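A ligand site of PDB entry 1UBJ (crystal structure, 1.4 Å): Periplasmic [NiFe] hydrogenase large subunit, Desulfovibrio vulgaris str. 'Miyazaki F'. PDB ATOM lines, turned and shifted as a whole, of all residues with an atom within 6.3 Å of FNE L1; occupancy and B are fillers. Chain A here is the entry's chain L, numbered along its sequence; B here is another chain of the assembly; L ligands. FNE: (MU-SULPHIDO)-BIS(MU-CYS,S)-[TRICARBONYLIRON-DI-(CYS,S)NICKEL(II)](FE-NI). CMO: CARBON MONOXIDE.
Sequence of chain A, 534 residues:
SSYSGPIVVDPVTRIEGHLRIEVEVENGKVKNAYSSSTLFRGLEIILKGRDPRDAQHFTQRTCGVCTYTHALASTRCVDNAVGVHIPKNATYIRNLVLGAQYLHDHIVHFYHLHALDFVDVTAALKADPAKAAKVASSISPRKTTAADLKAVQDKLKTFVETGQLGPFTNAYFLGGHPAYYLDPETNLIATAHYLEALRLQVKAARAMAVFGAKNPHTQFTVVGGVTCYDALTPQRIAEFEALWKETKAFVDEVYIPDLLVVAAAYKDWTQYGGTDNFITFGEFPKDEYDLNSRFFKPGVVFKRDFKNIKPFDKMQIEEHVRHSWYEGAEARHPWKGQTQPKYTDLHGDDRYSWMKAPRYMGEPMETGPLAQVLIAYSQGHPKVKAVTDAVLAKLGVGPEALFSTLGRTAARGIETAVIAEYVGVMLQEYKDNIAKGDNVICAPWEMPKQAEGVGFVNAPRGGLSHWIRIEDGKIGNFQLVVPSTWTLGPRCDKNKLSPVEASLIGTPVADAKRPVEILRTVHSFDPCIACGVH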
ATOM      1  N   GLU A  16      -0.696  -2.013 -28.068  1.00  0.00           N
ATOM      2  CA  GLU A  16      -1.061  -2.820 -26.927  1.00  0.00           C
ATOM      3  C   GLU A  16      -1.918  -3.995 -27.446  1.00  0.00           C
ATOM      4  O   GLU A  16      -2.925  -3.873 -28.096  1.00  0.00           O
ATOM      5  CB  GLU A  16      -1.818  -2.025 -25.876  1.00  0.00           C
ATOM      6  CG  GLU A  16      -1.951  -2.628 -24.504  1.00  0.00           C
ATOM      7  CD  GLU A  16      -2.818  -3.860 -24.387  1.00  0.00           C
ATOM      8  OE1 GLU A  16      -2.559  -4.884 -23.736  1.00  0.00           O
ATOM      9  OE2 GLU A  16      -3.770  -3.804 -25.262  1.00  0.00           O
ATOM     10  N   THR A  62      -8.209  -3.408 -17.378  1.00  0.00           N
ATOM     11  CA  THR A  62      -8.475  -3.591 -18.794  1.00  0.00           C
ATOM     12  C   THR A  62      -7.206  -3.290 -19.569  1.00  0.00           C
ATOM     13  O   THR A  62      -6.869  -3.921 -20.566  1.00  0.00           O
ATOM     14  CB  THR A  62      -9.592  -2.639 -19.266  1.00  0.00           C
ATOM     15  OG1 THR A  62     -10.850  -3.039 -18.662  1.00  0.00           O
ATOM     16  CG2 THR A  62      -9.789  -2.717 -20.776  1.00  0.00           C
ATOM     17  N   CYS A  63      -6.491  -2.229 -19.100  1.00  0.00           N
ATOM     18  CA  CYS A  63      -5.377  -1.742 -19.866  1.00  0.00           C
ATOM     19  C   CYS A  63      -4.408  -0.886 -19.026  1.00  0.00           C
ATOM     20  O   CYS A  63      -4.844   0.029 -18.316  1.00  0.00           O
ATOM     21  CB  CYS A  63      -5.870  -0.904 -21.023  1.00  0.00           C
ATOM     22  SG  CYS A  63      -4.478  -0.456 -22.173  1.00  0.00           S
ATOM     23  N   GLY A  64      -3.120  -1.253 -19.138  1.00  0.00           N
ATOM     24  CA  GLY A  64      -2.070  -0.501 -18.463  1.00  0.00           C
ATOM     25  C   GLY A  64      -1.332   0.523 -19.300  1.00  0.00           C
ATOM     26  O   GLY A  64      -0.490   1.252 -18.764  1.00  0.00           O
ATOM     27  N   VAL A  65      -1.633   0.585 -20.592  1.00  0.00           N
ATOM     28  CA  VAL A  65      -1.124   1.645 -21.456  1.00  0.00           C
ATOM     29  C   VAL A  65      -2.026   2.841 -21.241  1.00  0.00           C
ATOM     30  O   VAL A  65      -1.554   3.900 -20.797  1.00  0.00           O
ATOM     31  CB  VAL A  65      -1.070   1.216 -22.925  1.00  0.00           C
ATOM     32  CG1 VAL A  65      -0.674   2.379 -23.838  1.00  0.00           C
ATOM     33  CG2 VAL A  65      -0.121   0.031 -23.061  1.00  0.00           C
ATOM     34  N   CYS A  66      -3.351   2.676 -21.493  1.00  0.00           N
ATOM     35  CA  CYS A  66      -4.330   3.679 -21.122  1.00  0.00           C
ATOM     36  C   CYS A  66      -4.739   3.418 -19.672  1.00  0.00           C
ATOM     37  O   CYS A  66      -5.895   3.314 -19.294  1.00  0.00           O
ATOM     38  CB  CYS A  66      -5.489   3.755 -22.097  1.00  0.00           C
ATOM     39  SG  CYS A  66      -6.565   2.326 -22.166  1.00  0.00           S
ATOM     40  N   THR A  67      -3.719   3.305 -18.821  1.00  0.00           N
ATOM     41  CA  THR A  67      -3.931   3.219 -17.390  1.00  0.00           C
ATOM     42  C   THR A  67      -4.732   4.441 -16.927  1.00  0.00           C
ATOM     43  O   THR A  67      -4.849   5.437 -17.651  1.00  0.00           O
ATOM     44  CB  THR A  67      -2.599   3.047 -16.619  1.00  0.00           C
ATOM     45  OG1 THR A  67      -2.885   2.705 -15.274  1.00  0.00           O
ATOM     46  CG2 THR A  67      -1.794   4.336 -16.635  1.00  0.00           C
ATOM     47  N   THR A  69      -7.553   5.528 -17.199  1.00  0.00           N
ATOM     48  CA  THR A  69      -8.767   5.869 -17.955  1.00  0.00           C
ATOM     49  C   THR A  69      -9.970   5.019 -17.559  1.00  0.00           C
ATOM     50  O   THR A  69     -11.089   5.533 -17.395  1.00  0.00           O
ATOM     51  CB  THR A  69      -8.574   5.792 -19.490  1.00  0.00           C
ATOM     52  OG1 THR A  69      -8.352   4.425 -19.909  1.00  0.00           O
ATOM     53  CG2 THR A  69      -7.431   6.696 -19.972  1.00  0.00           C
ATOM     54  N   HIS A  70      -9.760   3.739 -17.333  1.00  0.00           N
ATOM     55  CA  HIS A  70     -10.877   2.864 -16.990  1.00  0.00           C
ATOM     56  C   HIS A  70     -11.286   3.005 -15.532  1.00  0.00           C
ATOM     57  O   HIS A  70     -12.474   2.849 -15.212  1.00  0.00           O
ATOM     58  CB  HIS A  70     -10.615   1.373 -17.321  1.00  0.00           C
ATOM     59  CG  HIS A  70     -10.514   1.118 -18.781  1.00  0.00           C
ATOM     60  ND1 HIS A  70     -11.647   0.880 -19.547  1.00  0.00           N
ATOM     61  CD2 HIS A  70      -9.449   1.066 -19.628  1.00  0.00           C
ATOM     62  CE1 HIS A  70     -11.267   0.676 -20.813  1.00  0.00           C
ATOM     63  NE2 HIS A  70      -9.924   0.791 -20.879  1.00  0.00           N
ATOM     64  N   ASP A 105       0.913   9.215 -22.877  1.00  0.00           N
ATOM     65  CA  ASP A 105       0.454   8.221 -23.854  1.00  0.00           C
ATOM     66  C   ASP A 105       0.801   8.592 -25.287  1.00  0.00           C
ATOM     67  O   ASP A 105       1.418   7.810 -26.036  1.00  0.00           O
ATOM     68  CB  ASP A 105      -1.056   8.023 -23.634  1.00  0.00           C
ATOM     69  CG  ASP A 105      -1.617   6.732 -24.151  1.00  0.00           C
ATOM     70  OD1 ASP A 105      -1.008   6.172 -25.110  1.00  0.00           O
ATOM     71  OD2 ASP A 105      -2.667   6.334 -23.573  1.00  0.00           O
ATOM     72  N   ALA A 459     -10.806   9.050 -23.926  1.00  0.00           N
ATOM     73  CA  ALA A 459      -9.478   8.543 -23.617  1.00  0.00           C
ATOM     74  C   ALA A 459      -8.508   8.894 -24.725  1.00  0.00           C
ATOM     75  O   ALA A 459      -8.957   9.437 -25.750  1.00  0.00           O
ATOM     76  CB  ALA A 459      -9.570   7.034 -23.365  1.00  0.00           C
ATOM     77  N   PRO A 460      -7.222   8.696 -24.581  1.00  0.00           N
ATOM     78  CA  PRO A 460      -6.299   9.013 -25.702  1.00  0.00           C
ATOM     79  C   PRO A 460      -6.651   8.302 -27.013  1.00  0.00           C
ATOM     80  O   PRO A 460      -6.204   8.804 -28.080  1.00  0.00           O
ATOM     81  CB  PRO A 460      -4.937   8.610 -25.119  1.00  0.00           C
ATOM     82  CG  PRO A 460      -5.123   8.835 -23.649  1.00  0.00           C
ATOM     83  CD  PRO A 460      -6.498   8.250 -23.374  1.00  0.00           C
ATOM     84  N   ARG A 461      -7.410   7.207 -27.009  1.00  0.00           N
ATOM     85  CA  ARG A 461      -7.828   6.535 -28.253  1.00  0.00           C
ATOM     86  C   ARG A 461      -9.286   6.769 -28.607  1.00  0.00           C
ATOM     87  O   ARG A 461      -9.807   6.300 -29.615  1.00  0.00           O
ATOM     88  CB  ARG A 461      -7.521   5.051 -28.122  1.00  0.00           C
ATOM     89  CG  ARG A 461      -6.000   4.787 -28.145  1.00  0.00           C
ATOM     90  CD  ARG A 461      -5.615   3.421 -27.543  1.00  0.00           C
ATOM     91  NE  ARG A 461      -4.163   3.418 -27.467  1.00  0.00           N
ATOM     92  CZ  ARG A 461      -3.479   4.060 -26.529  1.00  0.00           C
ATOM     93  NH1 ARG A 461      -4.096   4.727 -25.529  1.00  0.00           N
ATOM     94  NH2 ARG A 461      -2.165   4.026 -26.541  1.00  0.00           N
ATOM     95  N   GLY A 462     -10.002   7.555 -27.778  1.00  0.00           N
ATOM     96  CA  GLY A 462     -11.348   7.979 -28.088  1.00  0.00           C
ATOM     97  C   GLY A 462     -12.429   7.711 -27.068  1.00  0.00           C
ATOM     98  O   GLY A 462     -12.192   7.681 -25.863  1.00  0.00           O
ATOM     99  N   GLY A 463     -13.684   7.559 -27.521  1.00  0.00           N
ATOM    100  CA  GLY A 463     -14.796   7.546 -26.610  1.00  0.00           C
ATOM    101  C   GLY A 463     -14.958   6.236 -25.863  1.00  0.00           C
ATOM    102  O   GLY A 463     -15.302   5.212 -26.468  1.00  0.00           O
ATOM    103  N   LEU A 464     -14.743   6.350 -24.532  1.00  0.00           N
ATOM    104  CA  LEU A 464     -14.864   5.237 -23.619  1.00  0.00           C
ATOM    105  C   LEU A 464     -16.103   5.311 -22.763  1.00  0.00           C
ATOM    106  O   LEU A 464     -16.378   6.379 -22.228  1.00  0.00           O
ATOM    107  CB  LEU A 464     -13.640   5.205 -22.698  1.00  0.00           C
ATOM    108  CG  LEU A 464     -13.672   4.271 -21.510  1.00  0.00           C
ATOM    109  CD1 LEU A 464     -13.792   2.786 -21.935  1.00  0.00           C
ATOM    110  CD2 LEU A 464     -12.463   4.478 -20.617  1.00  0.00           C
ATOM    111  N   VAL A 482     -15.266   0.288 -25.553  1.00  0.00           N
ATOM    112  CA  VAL A 482     -13.961   0.979 -25.437  1.00  0.00           C
ATOM    113  C   VAL A 482     -13.575   1.583 -26.768  1.00  0.00           C
ATOM    114  O   VAL A 482     -14.040   1.062 -27.804  1.00  0.00           O
ATOM    115  CB  VAL A 482     -12.983  -0.064 -24.886  1.00  0.00           C
ATOM    116  CG1 VAL A 482     -11.642   0.486 -24.543  1.00  0.00           C
ATOM    117  CG2 VAL A 482     -13.511  -0.710 -23.595  1.00  0.00           C
ATOM    118  N   PRO A 483     -12.808   2.645 -26.851  1.00  0.00           N
ATOM    119  CA  PRO A 483     -12.480   3.264 -28.159  1.00  0.00           C
ATOM    120  C   PRO A 483     -11.925   2.267 -29.169  1.00  0.00           C
ATOM    121  O   PRO A 483     -12.395   2.279 -30.325  1.00  0.00           O
ATOM    122  CB  PRO A 483     -11.463   4.364 -27.846  1.00  0.00           C
ATOM    123  CG  PRO A 483     -11.257   4.321 -26.381  1.00  0.00           C
ATOM    124  CD  PRO A 483     -12.282   3.447 -25.755  1.00  0.00           C
ATOM    125  N   SER A 484     -10.992   1.391 -28.801  1.00  0.00           N
ATOM    126  CA  SER A 484     -10.501   0.462 -29.834  1.00  0.00           C
ATOM    127  C   SER A 484     -11.554  -0.558 -30.267  1.00  0.00           C
ATOM    128  O   SER A 484     -11.402  -1.133 -31.348  1.00  0.00           O
ATOM    129  CB  SER A 484      -9.239  -0.247 -29.365  1.00  0.00           C
ATOM    130  OG  SER A 484      -8.120   0.587 -29.262  1.00  0.00           O
ATOM    131  N   THR A 485     -12.566  -0.755 -29.450  1.00  0.00           N
ATOM    132  CA  THR A 485     -13.676  -1.610 -29.873  1.00  0.00           C
ATOM    133  C   THR A 485     -14.387  -0.968 -31.061  1.00  0.00           C
ATOM    134  O   THR A 485     -14.699  -1.648 -32.031  1.00  0.00           O
ATOM    135  CB  THR A 485     -14.714  -1.823 -28.743  1.00  0.00           C
ATOM    136  OG1 THR A 485     -14.070  -1.973 -27.472  1.00  0.00           O
ATOM    137  CG2 THR A 485     -15.575  -3.051 -29.000  1.00  0.00           C
ATOM    138  N   ASP A 526      -3.608   3.771 -33.242  1.00  0.00           N
ATOM    139  CA  ASP A 526      -3.107   3.472 -31.899  1.00  0.00           C
ATOM    140  C   ASP A 526      -3.936   2.398 -31.226  1.00  0.00           C
ATOM    141  O   ASP A 526      -4.565   2.572 -30.195  1.00  0.00           O
ATOM    142  CB  ASP A 526      -3.096   4.801 -31.155  1.00  0.00           C
ATOM    143  CG  ASP A 526      -2.494   4.826 -29.779  1.00  0.00           C
ATOM    144  OD1 ASP A 526      -2.704   5.875 -29.087  1.00  0.00           O
ATOM    145  OD2 ASP A 526      -1.876   3.802 -29.368  1.00  0.00           O
ATOM    146  N   PRO A 527      -3.931   1.196 -31.811  1.00  0.00           N
ATOM    147  CA  PRO A 527      -4.765   0.112 -31.323  1.00  0.00           C
ATOM    148  C   PRO A 527      -4.392  -0.356 -29.906  1.00  0.00           C
ATOM    149  O   PRO A 527      -3.225  -0.414 -29.525  1.00  0.00           O
ATOM    150  CB  PRO A 527      -4.489  -1.062 -32.267  1.00  0.00           C
ATOM    151  CG  PRO A 527      -3.968  -0.423 -33.497  1.00  0.00           C
ATOM    152  CD  PRO A 527      -3.161   0.765 -33.005  1.00  0.00           C
ATOM    153  N   CYS A 528      -5.455  -0.743 -29.191  1.00  0.00           N
ATOM    154  CA  CYS A 528      -5.326  -1.322 -27.872  1.00  0.00           C
ATOM    155  C   CYS A 528      -6.274  -2.508 -27.760  1.00  0.00           C
ATOM    156  O   CYS A 528      -7.467  -2.298 -27.631  1.00  0.00           O
ATOM    157  CB  CYS A 528      -5.554  -0.226 -26.815  1.00  0.00           C
ATOM    158  SG  CYS A 528      -5.264  -0.928 -25.164  1.00  0.00           S
ATOM    159  N   ILE A 529      -5.719  -3.716 -27.872  1.00  0.00           N
ATOM    160  CA  ILE A 529      -6.618  -4.883 -27.937  1.00  0.00           C
ATOM    161  C   ILE A 529      -7.089  -5.386 -26.589  1.00  0.00           C
ATOM    162  O   ILE A 529      -8.200  -5.943 -26.519  1.00  0.00           O
ATOM    163  CB  ILE A 529      -5.949  -6.002 -28.750  1.00  0.00           C
ATOM    164  CG1 ILE A 529      -5.284  -5.453 -30.004  1.00  0.00           C
ATOM    165  CG2 ILE A 529      -6.908  -7.108 -29.097  1.00  0.00           C
ATOM    166  CD1 ILE A 529      -6.131  -4.664 -30.967  1.00  0.00           C
ATOM    167  N   ALA A 530      -6.300  -5.152 -25.558  1.00  0.00           N
ATOM    168  CA  ALA A 530      -6.778  -5.415 -24.208  1.00  0.00           C
ATOM    169  C   ALA A 530      -7.963  -4.510 -23.872  1.00  0.00           C
ATOM    170  O   ALA A 530      -8.983  -4.985 -23.355  1.00  0.00           O
ATOM    171  CB  ALA A 530      -5.624  -5.219 -23.240  1.00  0.00           C
ATOM    172  N   CYS A 531      -7.870  -3.244 -24.215  1.00  0.00           N
ATOM    173  CA  CYS A 531      -8.996  -2.305 -24.186  1.00  0.00           C
ATOM    174  C   CYS A 531     -10.166  -2.783 -25.022  1.00  0.00           C
ATOM    175  O   CYS A 531     -11.315  -2.837 -24.606  1.00  0.00           O
ATOM    176  CB  CYS A 531      -8.537  -0.949 -24.772  1.00  0.00           C
ATOM    177  SG  CYS A 531      -7.974   0.130 -23.415  1.00  0.00           S
ATOM    178  N   GLY A 532      -9.851  -3.114 -26.290  1.00  0.00           N
ATOM    179  CA  GLY A 532     -10.953  -3.420 -27.188  1.00  0.00           C
ATOM    180  C   GLY A 532     -11.812  -4.597 -26.825  1.00  0.00           C
ATOM    181  O   GLY A 532     -13.053  -4.574 -27.007  1.00  0.00           O
ATOM    182  N   CYS B  17      -2.532  -6.823 -19.427  1.00  0.00           N
ATOM    183  CA  CYS B  17      -3.044  -5.497 -19.776  1.00  0.00           C
ATOM    184  C   CYS B  17      -1.953  -4.544 -20.221  1.00  0.00           C
ATOM    185  O   CYS B  17      -2.248  -3.410 -20.604  1.00  0.00           O
ATOM    186  CB  CYS B  17      -3.770  -4.924 -18.564  1.00  0.00           C
ATOM    187  SG  CYS B  17      -2.634  -4.205 -17.328  1.00  0.00           S
HETATM  188 NI   FNE L   1      -5.733   0.731 -23.648  1.00  0.00          NI
HETATM  189 FE   FNE L   1      -7.790   2.310 -24.043  1.00  0.00          FE
HETATM  190  C1  FNE L   1      -8.394   1.907 -25.853  1.00  0.00           C
HETATM  191  C2  FNE L   1      -7.243   4.004 -24.505  1.00  0.00           C
HETATM  192  C3  FNE L   1      -9.315   2.961 -23.502  1.00  0.00           C
HETATM  193  O1  FNE L   1      -8.735   1.703 -26.939  1.00  0.00           O
HETATM  194  O2  FNE L   1      -7.089   5.140 -24.786  1.00  0.00           O
HETATM  195  O3  FNE L   1     -10.303   3.362 -23.104  1.00  0.00           O
HETATM  196  C   CMO L   2      -4.517   1.698 -24.487  1.00  0.00           C
HETATM  197  O   CMO L   2      -3.513   1.709 -25.012  1.00  0.00           O
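OG1 of Thr 69 touches O3 of FNE L1 (3.9 Å). Ala 459 touches FNE L1. Pro 460 touches FNE L1 (CD to O2, 3.5 Å). CD2 of Leu 464 touches O3 of FNE L1, 3.5 Å away. Val 482 touches FNE L1 (CG1 to O3, 3.5 Å). CD of Pro 483 touches O3 of FNE L1 (3.3 Å). Hydrophobic or aromatic side chains within 4 Å of FNE L1: His 70, Ala 459, Pro 460, Leu 464, Val 482 and Pro 483. Of the 28 residues printed, 13 come within 4 Å of FNE L1.
FE of FNE L1 is bound by SG of Cys 66, at 2.2 Å. A nickel atom (NI) of FNE L1 is bound by the side-chain sulfur (SG) of Cys 63. The side-chain sulfur of Cys 531 is bound to an iron atom (FE) of FNE L1 (2.3 Å). SG of Cys 528 binds NI of FNE L1 (2.3 Å). N of Ser 484 is in hydrogen-bond range of O1 of FNE L1. OG of Ser 484 lies within hydrogen-bond range of O1 of FNE L1 (2.6 Å). The backbone NH of Arg 461 is in hydrogen-bond range of an oxygen (O2) of FNE L1 (3.1 Å). The guanidinium group (NH1) of Arg 461 lies within hydrogen-bond range of an oxygen (O2) of FNE L1, at 3.1 Å. A ring nitrogen (NE2) of His 70 is in hydrogen-bond range of an oxygen (O3) of FNE L1 (3.4 Å). The side-chain sulfur of Cys 63 lies close to an oxygen (O) of CMO L2 (3.7 Å). SG of Cys 528 lies close to O of CMO L2 (3.2 Å). NE of Arg 461 sits close to O of CMO L2, 3.1 Å away.
The side-chain hydroxyl of Thr 69 is in hydrogen-bond range of the backbone carbonyl oxygen of Cys 66 (2.8 Å). The backbone NH (N) of Val 65 lies close to the side-chain sulfur (SG) of Cys 63, 3.4 Å away. SG of Cys 531 sits close to NE2 of His 70. The backbone NH of Cys 528 sits at hydrogen-bond distance from the side-chain hydroxyl of Ser 484 (3.0 Å). SG of Cys 528 sits close to OE2 of Glu 16 (3.2 Å). The guanidinium group (NH2) of Arg 461 is in salt-bridge range of the side-chain carboxylate (OD1) of Asp 105, at 2.8 Å. The guanidinium group of Arg 461 lies within salt-bridge range of the side-chain carboxylate of Asp 526 (2.9 Å). The side-chain hydroxyl (OG1) of Thr 485 lies within hydrogen-bond range of the backbone carbonyl oxygen (O) of Val 482 (3.1 Å).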
